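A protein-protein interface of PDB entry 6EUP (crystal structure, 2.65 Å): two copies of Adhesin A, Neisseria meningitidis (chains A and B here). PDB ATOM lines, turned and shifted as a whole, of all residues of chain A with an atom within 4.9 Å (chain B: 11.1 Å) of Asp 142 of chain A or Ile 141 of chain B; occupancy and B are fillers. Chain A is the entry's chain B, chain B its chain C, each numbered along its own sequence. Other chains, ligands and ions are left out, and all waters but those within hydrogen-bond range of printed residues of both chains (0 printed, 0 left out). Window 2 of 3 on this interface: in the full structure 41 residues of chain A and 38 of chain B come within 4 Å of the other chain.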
ATOM      1  N   ILE A 138      28.858  24.098 -20.452  1.00  0.00           N
ATOM      2  CA  ILE A 138      28.131  23.241 -19.500  1.00  0.00           C
ATOM      3  C   ILE A 138      28.279  23.787 -18.066  1.00  0.00           C
ATOM      4  O   ILE A 138      27.314  23.758 -17.294  1.00  0.00           O
ATOM      5  CB  ILE A 138      28.539  21.745 -19.637  1.00  0.00           C
ATOM      6  CG1 ILE A 138      28.117  21.193 -21.001  1.00  0.00           C
ATOM      7  CG2 ILE A 138      27.984  20.877 -18.497  1.00  0.00           C
ATOM      8  CD1 ILE A 138      28.763  19.989 -21.340  1.00  0.00           C
ATOM      9  N   VAL A 139      29.457  24.350 -17.740  1.00  0.00           N
ATOM     10  CA  VAL A 139      29.674  24.914 -16.419  1.00  0.00           C
ATOM     11  C   VAL A 139      28.788  26.149 -16.222  1.00  0.00           C
ATOM     12  O   VAL A 139      28.115  26.246 -15.198  1.00  0.00           O
ATOM     13  CB  VAL A 139      31.168  25.143 -16.099  1.00  0.00           C
ATOM     14  CG1 VAL A 139      31.344  26.095 -14.908  1.00  0.00           C
ATOM     15  CG2 VAL A 139      31.871  23.805 -15.842  1.00  0.00           C
ATOM     16  N   LYS A 140      28.732  27.039 -17.226  1.00  0.00           N
ATOM     17  CA  LYS A 140      27.889  28.234 -17.216  1.00  0.00           C
ATOM     18  C   LYS A 140      26.413  27.845 -17.017  1.00  0.00           C
ATOM     19  O   LYS A 140      25.782  28.369 -16.084  1.00  0.00           O
ATOM     20  CB  LYS A 140      28.073  29.069 -18.490  1.00  0.00           C
ATOM     21  CG  LYS A 140      29.324  29.915 -18.466  1.00  0.00           C
ATOM     22  CD  LYS A 140      29.454  30.758 -19.737  1.00  0.00           C
ATOM     23  CE  LYS A 140      30.784  31.493 -19.821  1.00  0.00           C
ATOM     24  NZ  LYS A 140      31.297  31.585 -21.218  1.00  0.00           N
ATOM     25  N   ILE A 141      25.891  26.891 -17.831  1.00  0.00           N
ATOM     26  CA  ILE A 141      24.518  26.392 -17.704  1.00  0.00           C
ATOM     27  C   ILE A 141      24.299  25.900 -16.258  1.00  0.00           C
ATOM     28  O   ILE A 141      23.343  26.337 -15.615  1.00  0.00           O
ATOM     29  CB  ILE A 141      24.149  25.291 -18.741  1.00  0.00           C
ATOM     30  CG1 ILE A 141      24.117  25.813 -20.180  1.00  0.00           C
ATOM     31  CG2 ILE A 141      22.824  24.622 -18.382  1.00  0.00           C
ATOM     32  CD1 ILE A 141      24.477  24.777 -21.169  1.00  0.00           C
ATOM     33  N   ASP A 142      25.210  25.047 -15.737  1.00  0.00           N
ATOM     34  CA  ASP A 142      25.131  24.524 -14.365  1.00  0.00           C
ATOM     35  C   ASP A 142      25.001  25.640 -13.325  1.00  0.00           C
ATOM     36  O   ASP A 142      24.202  25.509 -12.402  1.00  0.00           O
ATOM     37  CB  ASP A 142      26.301  23.576 -14.035  1.00  0.00           C
ATOM     38  CG  ASP A 142      26.248  22.240 -14.759  1.00  0.00           C
ATOM     39  OD1 ASP A 142      25.217  21.949 -15.402  1.00  0.00           O
ATOM     40  OD2 ASP A 142      27.249  21.490 -14.698  1.00  0.00           O
ATOM     41  N   GLU A 143      25.728  26.749 -13.521  1.00  0.00           N
ATOM     42  CA  GLU A 143      25.694  27.923 -12.653  1.00  0.00           C
ATOM     43  C   GLU A 143      24.312  28.620 -12.716  1.00  0.00           C
ATOM     44  O   GLU A 143      23.714  28.851 -11.662  1.00  0.00           O
ATOM     45  CB  GLU A 143      26.849  28.887 -12.992  1.00  0.00           C
ATOM     46  CG  GLU A 143      28.205  28.404 -12.476  1.00  0.00           C
ATOM     47  CD  GLU A 143      29.452  29.218 -12.805  1.00  0.00           C
ATOM     48  OE1 GLU A 143      30.557  28.758 -12.431  1.00  0.00           O
ATOM     49  OE2 GLU A 143      29.337  30.310 -13.410  1.00  0.00           O
ATOM     50  N   LYS A 144      23.781  28.890 -13.945  1.00  0.00           N
ATOM     51  CA  LYS A 144      22.439  29.468 -14.167  1.00  0.00           C
ATOM     52  C   LYS A 144      21.358  28.586 -13.481  1.00  0.00           C
ATOM     53  O   LYS A 144      20.396  29.115 -12.920  1.00  0.00           O
ATOM     54  CB  LYS A 144      22.119  29.650 -15.668  1.00  0.00           C
ATOM     55  CG  LYS A 144      22.972  30.716 -16.392  1.00  0.00           C
ATOM     56  CD  LYS A 144      22.878  30.626 -17.951  1.00  0.00           C
ATOM     57  CE  LYS A 144      24.003  31.322 -18.724  1.00  0.00           C
ATOM     58  NZ  LYS A 144      23.967  31.035 -20.200  1.00  0.00           N
ATOM     59  N   LEU A 145      21.558  27.254 -13.471  1.00  0.00           N
ATOM     60  CA  LEU A 145      20.640  26.323 -12.814  1.00  0.00           C
ATOM     61  C   LEU A 145      20.792  26.329 -11.285  1.00  0.00           C
ATOM     62  O   LEU A 145      19.780  26.347 -10.590  1.00  0.00           O
ATOM     63  CB  LEU A 145      20.773  24.891 -13.370  1.00  0.00           C
ATOM     64  CG  LEU A 145      20.470  24.679 -14.849  1.00  0.00           C
ATOM     65  CD1 LEU A 145      20.665  23.234 -15.222  1.00  0.00           C
ATOM     66  CD2 LEU A 145      19.067  25.120 -15.211  1.00  0.00           C
ATOM     67  N   GLU A 146      22.046  26.308 -10.770  1.00  0.00           N
ATOM     68  CA  GLU A 146      22.380  26.311  -9.332  1.00  0.00           C
ATOM     69  C   GLU A 146      21.940  27.605  -8.651  1.00  0.00           C
ATOM     70  O   GLU A 146      21.609  27.593  -7.465  1.00  0.00           O
ATOM     71  CB  GLU A 146      23.888  26.079  -9.101  1.00  0.00           C
ATOM     72  CG  GLU A 146      24.305  24.616  -9.184  1.00  0.00           C
ATOM     73  CD  GLU A 146      25.789  24.321  -9.339  1.00  0.00           C
ATOM     74  OE1 GLU A 146      26.255  23.318  -8.751  1.00  0.00           O
ATOM     75  OE2 GLU A 146      26.482  25.064 -10.073  1.00  0.00           O
ATOM     76  N   GLU B 132      31.230  10.655 -23.907  1.00  0.00           N
ATOM     77  CA  GLU B 132      30.400  10.044 -22.862  1.00  0.00           C
ATOM     78  C   GLU B 132      30.060  11.025 -21.731  1.00  0.00           C
ATOM     79  O   GLU B 132      28.870  11.227 -21.448  1.00  0.00           O
ATOM     80  CB  GLU B 132      31.042   8.777 -22.315  1.00  0.00           C
ATOM     81  CG  GLU B 132      30.985   7.642 -23.308  1.00  0.00           C
ATOM     82  CD  GLU B 132      31.955   6.508 -23.034  1.00  0.00           C
ATOM     83  OE1 GLU B 132      31.527   5.335 -22.999  1.00  0.00           O
ATOM     84  OE2 GLU B 132      33.161   6.793 -22.895  1.00  0.00           O
ATOM     85  N   GLU B 133      31.083  11.674 -21.121  1.00  0.00           N
ATOM     86  CA  GLU B 133      30.856  12.643 -20.041  1.00  0.00           C
ATOM     87  C   GLU B 133      29.966  13.779 -20.515  1.00  0.00           C
ATOM     88  O   GLU B 133      29.039  14.143 -19.797  1.00  0.00           O
ATOM     89  CB  GLU B 133      32.171  13.174 -19.436  1.00  0.00           C
ATOM     90  CG  GLU B 133      33.005  12.127 -18.708  1.00  0.00           C
ATOM     91  CD  GLU B 133      34.504  12.394 -18.580  1.00  0.00           C
ATOM     92  OE1 GLU B 133      35.134  11.799 -17.672  1.00  0.00           O
ATOM     93  OE2 GLU B 133      35.057  13.172 -19.391  1.00  0.00           O
ATOM     94  N   THR B 134      30.168  14.290 -21.747  1.00  0.00           N
ATOM     95  CA  THR B 134      29.318  15.341 -22.312  1.00  0.00           C
ATOM     96  C   THR B 134      27.852  14.881 -22.457  1.00  0.00           C
ATOM     97  O   THR B 134      26.923  15.641 -22.137  1.00  0.00           O
ATOM     98  CB  THR B 134      29.908  15.797 -23.621  1.00  0.00           C
ATOM     99  OG1 THR B 134      31.210  16.286 -23.344  1.00  0.00           O
ATOM    100  CG2 THR B 134      29.092  16.869 -24.289  1.00  0.00           C
ATOM    101  N   LYS B 135      27.642  13.644 -22.921  1.00  0.00           N
ATOM    102  CA  LYS B 135      26.284  13.130 -23.086  1.00  0.00           C
ATOM    103  C   LYS B 135      25.603  13.101 -21.738  1.00  0.00           C
ATOM    104  O   LYS B 135      24.500  13.615 -21.623  1.00  0.00           O
ATOM    105  CB  LYS B 135      26.277  11.754 -23.767  1.00  0.00           C
ATOM    106  CG  LYS B 135      24.877  11.277 -24.099  1.00  0.00           C
ATOM    107  CD  LYS B 135      24.809   9.799 -24.402  1.00  0.00           C
ATOM    108  CE  LYS B 135      23.386   9.357 -24.663  1.00  0.00           C
ATOM    109  NZ  LYS B 135      23.323   7.929 -25.075  1.00  0.00           N
ATOM    110  N   THR B 136      26.312  12.620 -20.697  1.00  0.00           N
ATOM    111  CA  THR B 136      25.828  12.515 -19.336  1.00  0.00           C
ATOM    112  C   THR B 136      25.421  13.875 -18.782  1.00  0.00           C
ATOM    113  O   THR B 136      24.325  14.001 -18.215  1.00  0.00           O
ATOM    114  CB  THR B 136      26.859  11.771 -18.500  1.00  0.00           C
ATOM    115  OG1 THR B 136      26.724  10.371 -18.764  1.00  0.00           O
ATOM    116  CG2 THR B 136      26.711  12.020 -17.010  1.00  0.00           C
ATOM    117  N   ASN B 137      26.278  14.893 -18.958  1.00  0.00           N
ATOM    118  CA  ASN B 137      25.968  16.209 -18.444  1.00  0.00           C
ATOM    119  C   ASN B 137      24.774  16.832 -19.113  1.00  0.00           C
ATOM    120  O   ASN B 137      23.911  17.334 -18.404  1.00  0.00           O
ATOM    121  CB  ASN B 137      27.162  17.107 -18.488  1.00  0.00           C
ATOM    122  CG  ASN B 137      28.246  16.685 -17.569  1.00  0.00           C
ATOM    123  OD1 ASN B 137      28.043  15.891 -16.650  1.00  0.00           O
ATOM    124  ND2 ASN B 137      29.433  17.212 -17.802  1.00  0.00           N
ATOM    125  N   ILE B 138      24.689  16.773 -20.457  1.00  0.00           N
ATOM    126  CA  ILE B 138      23.563  17.339 -21.227  1.00  0.00           C
ATOM    127  C   ILE B 138      22.263  16.641 -20.855  1.00  0.00           C
ATOM    128  O   ILE B 138      21.243  17.298 -20.714  1.00  0.00           O
ATOM    129  CB  ILE B 138      23.848  17.370 -22.752  1.00  0.00           C
ATOM    130  CG1 ILE B 138      25.006  18.332 -23.046  1.00  0.00           C
ATOM    131  CG2 ILE B 138      22.618  17.772 -23.551  1.00  0.00           C
ATOM    132  CD1 ILE B 138      25.606  18.145 -24.349  1.00  0.00           C
ATOM    133  N   VAL B 139      22.327  15.324 -20.603  1.00  0.00           N
ATOM    134  CA  VAL B 139      21.180  14.511 -20.189  1.00  0.00           C
ATOM    135  C   VAL B 139      20.687  14.971 -18.824  1.00  0.00           C
ATOM    136  O   VAL B 139      19.489  15.198 -18.686  1.00  0.00           O
ATOM    137  CB  VAL B 139      21.491  13.006 -20.267  1.00  0.00           C
ATOM    138  CG1 VAL B 139      20.551  12.194 -19.389  1.00  0.00           C
ATOM    139  CG2 VAL B 139      21.445  12.528 -21.720  1.00  0.00           C
ATOM    140  N   LYS B 140      21.613  15.181 -17.855  1.00  0.00           N
ATOM    141  CA  LYS B 140      21.316  15.680 -16.508  1.00  0.00           C
ATOM    142  C   LYS B 140      20.638  17.066 -16.599  1.00  0.00           C
ATOM    143  O   LYS B 140      19.555  17.228 -16.016  1.00  0.00           O
ATOM    144  CB  LYS B 140      22.582  15.766 -15.638  1.00  0.00           C
ATOM    145  CG  LYS B 140      23.039  14.447 -15.067  1.00  0.00           C
ATOM    146  CD  LYS B 140      24.361  14.644 -14.318  1.00  0.00           C
ATOM    147  CE  LYS B 140      24.909  13.377 -13.713  1.00  0.00           C
ATOM    148  NZ  LYS B 140      26.369  13.481 -13.487  1.00  0.00           N
ATOM    149  N   ILE B 141      21.251  18.042 -17.340  1.00  0.00           N
ATOM    150  CA  ILE B 141      20.688  19.384 -17.544  1.00  0.00           C
ATOM    151  C   ILE B 141      19.259  19.243 -18.102  1.00  0.00           C
ATOM    152  O   ILE B 141      18.332  19.810 -17.523  1.00  0.00           O
ATOM    153  CB  ILE B 141      21.558  20.291 -18.465  1.00  0.00           C
ATOM    154  CG1 ILE B 141      22.874  20.711 -17.787  1.00  0.00           C
ATOM    155  CG2 ILE B 141      20.768  21.510 -18.960  1.00  0.00           C
ATOM    156  CD1 ILE B 141      23.979  20.876 -18.706  1.00  0.00           C
ATOM    157  N   ASP B 142      19.081  18.468 -19.196  1.00  0.00           N
ATOM    158  CA  ASP B 142      17.768  18.250 -19.796  1.00  0.00           C
ATOM    159  C   ASP B 142      16.756  17.755 -18.752  1.00  0.00           C
ATOM    160  O   ASP B 142      15.653  18.288 -18.717  1.00  0.00           O
ATOM    161  CB  ASP B 142      17.839  17.341 -21.034  1.00  0.00           C
ATOM    162  CG  ASP B 142      18.589  17.929 -22.220  1.00  0.00           C
ATOM    163  OD1 ASP B 142      18.902  19.130 -22.187  1.00  0.00           O
ATOM    164  OD2 ASP B 142      18.902  17.167 -23.168  1.00  0.00           O
ATOM    165  N   GLU B 143      17.161  16.834 -17.853  1.00  0.00           N
ATOM    166  CA  GLU B 143      16.317  16.305 -16.777  1.00  0.00           C
ATOM    167  C   GLU B 143      15.895  17.418 -15.791  1.00  0.00           C
ATOM    168  O   GLU B 143      14.695  17.556 -15.530  1.00  0.00           O
ATOM    169  CB  GLU B 143      16.993  15.125 -16.052  1.00  0.00           C
ATOM    170  CG  GLU B 143      16.940  13.828 -16.854  1.00  0.00           C
ATOM    171  CD  GLU B 143      17.663  12.594 -16.334  1.00  0.00           C
ATOM    172  OE1 GLU B 143      17.913  12.483 -15.109  1.00  0.00           O
ATOM    173  OE2 GLU B 143      17.921  11.694 -17.167  1.00  0.00           O
ATOM    174  N   LYS B 144      16.865  18.237 -15.295  1.00  0.00           N
ATOM    175  CA  LYS B 144      16.608  19.386 -14.410  1.00  0.00           C
ATOM    176  C   LYS B 144      15.618  20.370 -15.099  1.00  0.00           C
ATOM    177  O   LYS B 144      14.760  20.942 -14.422  1.00  0.00           O
ATOM    178  CB  LYS B 144      17.912  20.120 -14.020  1.00  0.00           C
ATOM    179  CG  LYS B 144      18.866  19.319 -13.111  1.00  0.00           C
ATOM    180  CD  LYS B 144      20.299  19.945 -13.031  1.00  0.00           C
ATOM    181  CE  LYS B 144      21.400  19.011 -12.521  1.00  0.00           C
ATOM    182  NZ  LYS B 144      22.768  19.599 -12.667  1.00  0.00           N
ATOM    183  N   LEU B 145      15.699  20.511 -16.442  1.00  0.00           N
ATOM    184  CA  LEU B 145      14.788  21.366 -17.198  1.00  0.00           C
ATOM    185  C   LEU B 145      13.402  20.725 -17.381  1.00  0.00           C
ATOM    186  O   LEU B 145      12.406  21.424 -17.220  1.00  0.00           O
ATOM    187  CB  LEU B 145      15.372  21.776 -18.558  1.00  0.00           C
ATOM    188  CG  LEU B 145      16.668  22.583 -18.562  1.00  0.00           C
ATOM    189  CD1 LEU B 145      17.081  22.898 -19.971  1.00  0.00           C
ATOM    190  CD2 LEU B 145      16.538  23.872 -17.778  1.00  0.00           C
ATOM    191  N   GLU B 146      13.340  19.410 -17.721  1.00  0.00           N
ATOM    192  CA  GLU B 146      12.099  18.639 -17.934  1.00  0.00           C
ATOM    193  C   GLU B 146      11.287  18.513 -16.644  1.00  0.00           C
ATOM    194  O   GLU B 146      10.057  18.432 -16.699  1.00  0.00           O
ATOM    195  CB  GLU B 146      12.396  17.248 -18.516  1.00  0.00           C
ATOM    196  CG  GLU B 146      12.653  17.244 -20.018  1.00  0.00           C
ATOM    197  CD  GLU B 146      13.308  16.006 -20.617  1.00  0.00           C
ATOM    198  OE1 GLU B 146      13.037  15.718 -21.805  1.00  0.00           O
ATOM    199  OE2 GLU B 146      14.125  15.351 -19.924  1.00  0.00           O
ATOM    200  N   ALA B 147      11.983  18.504 -15.490  1.00  0.00           N
ATOM    201  CA  ALA B 147      11.376  18.440 -14.165  1.00  0.00           C
ATOM    202  C   ALA B 147      10.868  19.823 -13.758  1.00  0.00           C
ATOM    203  O   ALA B 147       9.718  19.932 -13.342  1.00  0.00           O
ATOM    204  CB  ALA B 147      12.379  17.924 -13.147  1.00  0.00           C
ATOM    205  N   ALA B 148      11.703  20.881 -13.909  1.00  0.00           N
ATOM    206  CA  ALA B 148      11.339  22.271 -13.586  1.00  0.00           C
ATOM    207  C   ALA B 148      10.157  22.801 -14.430  1.00  0.00           C
ATOM    208  O   ALA B 148       9.496  23.754 -14.009  1.00  0.00           O
ATOM    209  CB  ALA B 148      12.551  23.191 -13.711  1.00  0.00           C
ATOM    210  N   SER B 149       9.872  22.167 -15.592  1.00  0.00           N
ATOM    211  CA  SER B 149       8.751  22.521 -16.474  1.00  0.00           C
ATOM    212  C   SER B 149       7.435  22.009 -15.868  1.00  0.00           C
ATOM    213  O   SER B 149       6.449  22.752 -15.822  1.00  0.00           O
ATOM    214  CB  SER B 149       8.954  21.940 -17.869  1.00  0.00           C
ATOM    215  OG  SER B 149       8.001  22.460 -18.782  1.00  0.00           O
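Ile 141 of chain A touches its own counterpart, Ile 141 of chain B.
Asp 142 of chain A touches Ile 141 of chain B, but with the chains exchanged Ile 141 of chain A does not touch Asp 142 of chain B (7.2 Å).
Leu 145 of chain A touches Lys 144 of chain B, but with the chains exchanged Lys 144 of chain A does not touch Leu 145 of chain B (8.0 Å).
Leu 145 of chain B touches its own counterpart, Leu 145 of chain A.
Of the 5 pairs that touch across the chains among the printed residues, 2 have their exchanged pair printed and touching as well.
Of the printed residues of chain B, Asp 142 of chain A touches Ile 141 (3.6 Å).
Of the printed residues of chain A, Ile 141 of chain B touches Ile 141 and Asp 142.
No residue of chain B comes within 4 Å of Val 139 of chain A.
Leu 145 of chain A touches two residues of chain B.
No residue of chain B comes within 4 Å of Glu 146 of chain A.
Of the printed residues of chain B, Ile 138 of chain A touches Asn 137 (3.9 Å).
Of the printed residues of chain A, Lys 144 of chain B touches Leu 145.
The nearest residue of chain B that does not touch Asp 142 of chain A is Lys 144 of chain B (4.4 Å).
The nearest printed residue of chain A that does not touch Leu 145 of chain B is Ile 141 of chain A (6.2 Å).
Of the 18 printed residues of chain B, 4 touch a printed residue of chain A.
Hydrophobic or aromatic side chains of chain B that line the printed part of chain A: Ile 141 and Leu 145.
Hydrophobic or aromatic side chains of chain A within 4 Å of the printed part of chain B: Ile 138, Ile 141 and Leu 145.
Among the printed residues, no Asp or Glu carboxylate lies within 4 Å of a Lys or Arg side-chain nitrogen of the other chain.
Among the printed residues, merely in contact across the chains: Asp 142 of chain A with Ile 141 of chain B (3.6 Å), Ile 141 of chain A with Ile 141 of chain B (3.8 Å), Leu 145 of chain A with Leu 145 of chain B (3.8 Å), Ile 138 of chain A with Asn 137 of chain B (3.9 Å) and Leu 145 of chain A with Lys 144 of chain B (3.97 Å).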
